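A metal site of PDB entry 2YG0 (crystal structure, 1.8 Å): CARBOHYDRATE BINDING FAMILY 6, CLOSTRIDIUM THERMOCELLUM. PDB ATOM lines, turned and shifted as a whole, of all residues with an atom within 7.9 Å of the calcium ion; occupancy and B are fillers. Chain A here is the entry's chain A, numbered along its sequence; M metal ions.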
ATOM      1  N   THR A  24       3.489 -26.183   1.053  1.00  0.00           N
ATOM      2  CA  THR A  24       3.019 -24.887   1.624  1.00  0.00           C
ATOM      3  C   THR A  24       3.937 -24.516   2.802  1.00  0.00           C
ATOM      4  O   THR A  24       4.849 -25.294   3.213  1.00  0.00           O
ATOM      5  CB  THR A  24       1.606 -25.045   2.193  1.00  0.00           C
ATOM      6  OG1 THR A  24       1.694 -26.014   3.258  1.00  0.00           O
ATOM      7  CG2 THR A  24       0.638 -25.578   1.103  1.00  0.00           C
ATOM      8  N   ILE A  25       3.674 -23.366   3.390  1.00  0.00           N
ATOM      9  CA  ILE A  25       4.453 -22.893   4.559  1.00  0.00           C
ATOM     10  C   ILE A  25       4.477 -23.902   5.699  1.00  0.00           C
ATOM     11  O   ILE A  25       5.397 -23.916   6.483  1.00  0.00           O
ATOM     12  CB  ILE A  25       3.955 -21.557   5.090  1.00  0.00           C
ATOM     13  CG1 ILE A  25       2.435 -21.625   5.389  1.00  0.00           C
ATOM     14  CG2 ILE A  25       4.255 -20.497   3.982  1.00  0.00           C
ATOM     15  CD1 ILE A  25       1.819 -20.229   5.874  1.00  0.00           C
ATOM     16  N   HIS A  26       3.437 -24.738   5.821  1.00  0.00           N
ATOM     17  CA  HIS A  26       3.395 -25.687   6.903  1.00  0.00           C
ATOM     18  C   HIS A  26       4.539 -26.691   6.870  1.00  0.00           C
ATOM     19  O   HIS A  26       4.871 -27.242   7.921  1.00  0.00           O
ATOM     20  CB  HIS A  26       2.025 -26.432   6.904  1.00  0.00           C
ATOM     21  CG  HIS A  26       0.884 -25.502   7.181  1.00  0.00           C
ATOM     22  ND1 HIS A  26       0.544 -25.115   8.456  1.00  0.00           N
ATOM     23  CD2 HIS A  26       0.124 -24.750   6.326  1.00  0.00           C
ATOM     24  CE1 HIS A  26      -0.415 -24.197   8.391  1.00  0.00           C
ATOM     25  NE2 HIS A  26      -0.681 -23.955   7.117  1.00  0.00           N
ATOM     26  N   LYS A  27       5.138 -26.916   5.710  1.00  0.00           N
ATOM     27  CA  LYS A  27       6.280 -27.843   5.631  1.00  0.00           C
ATOM     28  C   LYS A  27       7.505 -27.321   6.366  1.00  0.00           C
ATOM     29  O   LYS A  27       8.453 -28.097   6.653  1.00  0.00           O
ATOM     30  CB  LYS A  27       6.672 -28.114   4.190  1.00  0.00           C
ATOM     31  CG  LYS A  27       5.548 -28.585   3.274  1.00  0.00           C
ATOM     32  CD  LYS A  27       4.919 -29.870   3.856  1.00  0.00           C
ATOM     33  CE  LYS A  27       3.944 -30.476   2.833  1.00  0.00           C
ATOM     34  NZ  LYS A  27       2.905 -31.353   3.526  1.00  0.00           N
ATOM     35  N   ALA A  28       7.526 -26.047   6.733  1.00  0.00           N
ATOM     36  CA  ALA A  28       8.684 -25.529   7.461  1.00  0.00           C
ATOM     37  C   ALA A  28       8.559 -25.758   8.961  1.00  0.00           C
ATOM     38  O   ALA A  28       9.477 -25.413   9.721  1.00  0.00           O
ATOM     39  CB  ALA A  28       8.869 -23.993   7.151  1.00  0.00           C
ATOM     40  N   PHE A  29       7.471 -26.414   9.409  1.00  0.00           N
ATOM     41  CA  PHE A  29       7.272 -26.563  10.852  1.00  0.00           C
ATOM     42  C   PHE A  29       6.973 -28.000  11.252  1.00  0.00           C
ATOM     43  O   PHE A  29       6.478 -28.240  12.371  1.00  0.00           O
ATOM     44  CB  PHE A  29       6.121 -25.671  11.334  1.00  0.00           C
ATOM     45  CG  PHE A  29       6.337 -24.213  11.003  1.00  0.00           C
ATOM     46  CD1 PHE A  29       7.034 -23.365  11.901  1.00  0.00           C
ATOM     47  CD2 PHE A  29       5.866 -23.693   9.784  1.00  0.00           C
ATOM     48  CE1 PHE A  29       7.220 -21.985  11.574  1.00  0.00           C
ATOM     49  CE2 PHE A  29       6.065 -22.312   9.468  1.00  0.00           C
ATOM     50  CZ  PHE A  29       6.722 -21.473  10.370  1.00  0.00           C
ATOM     51  N   ASP A  30       7.207 -28.918  10.336  1.00  0.00           N
ATOM     52  CA  ASP A  30       6.762 -30.293  10.536  1.00  0.00           C
ATOM     53  C   ASP A  30       7.846 -31.195  11.142  1.00  0.00           C
ATOM     54  O   ASP A  30       7.601 -32.390  11.296  1.00  0.00           O
ATOM     55  CB  ASP A  30       6.302 -30.946   9.221  1.00  0.00           C
ATOM     56  CG  ASP A  30       7.336 -30.973   8.143  1.00  0.00           C
ATOM     57  OD1 ASP A  30       8.516 -30.512   8.301  1.00  0.00           O
ATOM     58  OD2 ASP A  30       6.957 -31.426   7.031  1.00  0.00           O
ATOM     59  N   GLY A  31       9.003 -30.643  11.424  1.00  0.00           N
ATOM     60  CA  GLY A  31      10.118 -31.467  12.025  1.00  0.00           C
ATOM     61  C   GLY A  31      10.916 -32.285  11.024  1.00  0.00           C
ATOM     62  O   GLY A  31      11.845 -33.011  11.421  1.00  0.00           O
ATOM     63  N   ASP A  32      10.602 -32.230   9.751  1.00  0.00           N
ATOM     64  CA  ASP A  32      11.338 -33.049   8.774  1.00  0.00           C
ATOM     65  C   ASP A  32      12.216 -32.113   7.949  1.00  0.00           C
ATOM     66  O   ASP A  32      11.667 -31.177   7.289  1.00  0.00           O
ATOM     67  CB  ASP A  32      10.318 -33.735   7.878  1.00  0.00           C
ATOM     68  CG  ASP A  32      10.936 -34.721   6.927  1.00  0.00           C
ATOM     69  OD1 ASP A  32      12.163 -34.770   6.823  1.00  0.00           O
ATOM     70  OD2 ASP A  32      10.188 -35.452   6.274  1.00  0.00           O
ATOM     71  N   LEU A  33      13.529 -32.299   7.984  1.00  0.00           N
ATOM     72  CA  LEU A  33      14.418 -31.423   7.230  1.00  0.00           C
ATOM     73  C   LEU A  33      14.344 -31.713   5.735  1.00  0.00           C
ATOM     74  O   LEU A  33      14.874 -30.942   4.931  1.00  0.00           O
ATOM     75  CB  LEU A  33      15.858 -31.536   7.735  1.00  0.00           C
ATOM     76  CG  LEU A  33      16.050 -31.315   9.258  1.00  0.00           C
ATOM     77  CD1 LEU A  33      17.603 -31.320   9.555  1.00  0.00           C
ATOM     78  CD2 LEU A  33      15.387 -29.952   9.672  1.00  0.00           C
ATOM     79  N   ASN A  34      13.701 -32.836   5.371  1.00  0.00           N
ATOM     80  CA  ASN A  34      13.567 -33.174   3.955  1.00  0.00           C
ATOM     81  C   ASN A  34      12.352 -32.486   3.287  1.00  0.00           C
ATOM     82  O   ASN A  34      12.219 -32.528   2.065  1.00  0.00           O
ATOM     83  CB  ASN A  34      13.339 -34.676   3.788  1.00  0.00           C
ATOM     84  CG  ASN A  34      14.485 -35.475   4.377  1.00  0.00           C
ATOM     85  OD1 ASN A  34      14.329 -36.148   5.422  1.00  0.00           O
ATOM     86  ND2 ASN A  34      15.655 -35.311   3.802  1.00  0.00           N
ATOM     87  N   THR A  35      11.445 -31.957   4.084  1.00  0.00           N
ATOM     88  CA  THR A  35      10.282 -31.292   3.492  1.00  0.00           C
ATOM     89  C   THR A  35      10.458 -29.800   3.566  1.00  0.00           C
ATOM     90  O   THR A  35      11.025 -29.286   4.545  1.00  0.00           O
ATOM     91  CB  THR A  35       8.979 -31.590   4.243  1.00  0.00           C
ATOM     92  OG1 THR A  35       9.112 -31.171   5.622  1.00  0.00           O
ATOM     93  CG2 THR A  35       8.611 -33.079   4.173  1.00  0.00           C
ATOM     94  N   PHE A  36       9.918 -29.073   2.594  1.00  0.00           N
ATOM     95  CA  PHE A  36      10.285 -27.664   2.513  1.00  0.00           C
ATOM     96  C   PHE A  36       9.075 -26.884   1.990  1.00  0.00           C
ATOM     97  O   PHE A  36       8.188 -27.452   1.355  1.00  0.00           O
ATOM     98  CB  PHE A  36      11.487 -27.448   1.516  1.00  0.00           C
ATOM     99  CG  PHE A  36      11.276 -28.140   0.179  1.00  0.00           C
ATOM    100  CD1 PHE A  36      10.564 -27.513  -0.852  1.00  0.00           C
ATOM    101  CD2 PHE A  36      11.723 -29.468   0.009  1.00  0.00           C
ATOM    102  CE1 PHE A  36      10.326 -28.184  -2.077  1.00  0.00           C
ATOM    103  CE2 PHE A  36      11.481 -30.143  -1.193  1.00  0.00           C
ATOM    104  CZ  PHE A  36      10.774 -29.498  -2.220  1.00  0.00           C
ATOM    105  N   PHE A  37       9.096 -25.590   2.260  1.00  0.00           N
ATOM    106  CA  PHE A  37       8.169 -24.615   1.649  1.00  0.00           C
ATOM    107  C   PHE A  37       8.704 -24.202   0.283  1.00  0.00           C
ATOM    108  O   PHE A  37       9.894 -23.811   0.164  1.00  0.00           O
ATOM    109  CB  PHE A  37       8.069 -23.394   2.574  1.00  0.00           C
ATOM    110  CG  PHE A  37       7.342 -22.217   1.962  1.00  0.00           C
ATOM    111  CD1 PHE A  37       6.131 -22.407   1.315  1.00  0.00           C
ATOM    112  CD2 PHE A  37       7.852 -20.915   2.125  1.00  0.00           C
ATOM    113  CE1 PHE A  37       5.402 -21.291   0.765  1.00  0.00           C
ATOM    114  CE2 PHE A  37       7.141 -19.786   1.579  1.00  0.00           C
ATOM    115  CZ  PHE A  37       5.920 -19.997   0.898  1.00  0.00           C
ATOM    116  N   CYS A  65      16.789 -24.483   8.481  1.00  0.00           N
ATOM    117  CA  CYS A  65      17.494 -25.423   7.605  1.00  0.00           C
ATOM    118  C   CYS A  65      17.008 -25.069   6.198  1.00  0.00           C
ATOM    119  O   CYS A  65      15.797 -24.901   5.992  1.00  0.00           O
ATOM    120  CB  CYS A  65      17.059 -26.857   7.964  1.00  0.00           C
ATOM    121  SG  CYS A  65      17.724 -28.116   6.785  1.00  0.00           S
ATOM    122  N   ILE A 131      12.716 -22.848   2.167  1.00  0.00           N
ATOM    123  CA  ILE A 131      13.305 -23.142   3.465  1.00  0.00           C
ATOM    124  C   ILE A 131      12.711 -24.466   3.888  1.00  0.00           C
ATOM    125  O   ILE A 131      11.536 -24.740   3.644  1.00  0.00           O
ATOM    126  CB  ILE A 131      12.932 -22.003   4.503  1.00  0.00           C
ATOM    127  CG1 ILE A 131      13.537 -22.239   5.884  1.00  0.00           C
ATOM    128  CG2 ILE A 131      11.354 -21.768   4.586  1.00  0.00           C
ATOM    129  CD1 ILE A 131      13.301 -21.050   6.884  1.00  0.00           C
ATOM    130  N   ALA A 132      13.510 -25.315   4.534  1.00  0.00           N
ATOM    131  CA  ALA A 132      12.974 -26.618   4.956  1.00  0.00           C
ATOM    132  C   ALA A 132      12.415 -26.631   6.336  1.00  0.00           C
ATOM    133  O   ALA A 132      11.469 -27.362   6.627  1.00  0.00           O
ATOM    134  CB  ALA A 132      14.084 -27.762   4.847  1.00  0.00           C
ATOM    135  N   GLU A 133      13.014 -25.860   7.239  1.00  0.00           N
ATOM    136  CA  GLU A 133      12.517 -25.917   8.604  1.00  0.00           C
ATOM    137  C   GLU A 133      12.879 -24.616   9.313  1.00  0.00           C
ATOM    138  O   GLU A 133      13.934 -24.018   9.080  1.00  0.00           O
ATOM    139  CB  GLU A 133      13.182 -27.121   9.374  1.00  0.00           C
ATOM    140  CG  GLU A 133      12.346 -27.553  10.582  1.00  0.00           C
ATOM    141  CD  GLU A 133      11.054 -28.286  10.234  1.00  0.00           C
ATOM    142  OE1 GLU A 133      10.880 -28.829   9.101  1.00  0.00           O
ATOM    143  OE2 GLU A 133      10.220 -28.347  11.137  1.00  0.00           O
ATOM    144  N   LEU A 134      11.994 -24.203  10.207  1.00  0.00           N
ATOM    145  CA  LEU A 134      12.140 -22.904  10.857  1.00  0.00           C
ATOM    146  C   LEU A 134      11.672 -23.041  12.281  1.00  0.00           C
ATOM    147  O   LEU A 134      10.550 -23.541  12.514  1.00  0.00           O
ATOM    148  CB  LEU A 134      11.235 -21.872  10.119  1.00  0.00           C
ATOM    149  CG  LEU A 134      11.166 -20.488  10.791  1.00  0.00           C
ATOM    150  CD1 LEU A 134      12.558 -19.860  10.887  1.00  0.00           C
ATOM    151  CD2 LEU A 134      10.209 -19.564   9.962  1.00  0.00           C
HETATM  152 CA    CA M   1      10.258 -29.420   6.969  1.00  0.00          CA
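The side-chain carboxylate (OD1) of Asp 32 is in hydrogen-bond range of the backbone NH (N) of Asn 34. The backbone NH (N) of Gly 31 sits at hydrogen-bond distance from the side-chain carboxylate (OE2) of Glu 133 (2.6 Å). O of Glu 133 is in hydrogen-bond range of N of Cys 65. O of Cys 65 lies within hydrogen-bond range of N of Ala 132, at 2.7 Å.
Six residues have an atom within 4 Å of the calcium ion: Lys 27, Asp 30, Asp 32, Thr 35, Ala 132 and Glu 133. The nearest printed residue that does not touch the calcium ion is Ala 28 (4.2 Å).
The calcium ion is bound by the backbone carbonyl oxygen (O) of Lys 27, 2.3 Å away. The backbone carbonyl oxygen (O) of Asp 32 binds the calcium ion (2.3 Å). The calcium ion is bound by OE1 of Glu 133, 2.3 Å away. The backbone carbonyl oxygen (O) of Ala 132 is bound to the calcium ion, at 2.4 Å. The calcium ion is bound by OD1 of Asp 30, at 2.4 Å. OG1 of Thr 35 is bound to the calcium ion (2.5 Å). The calcium ion is bound by the backbone carbonyl oxygen (O) of Thr 35, 2.5 Å away. The calcium ion has seven donor atoms within binding distance.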
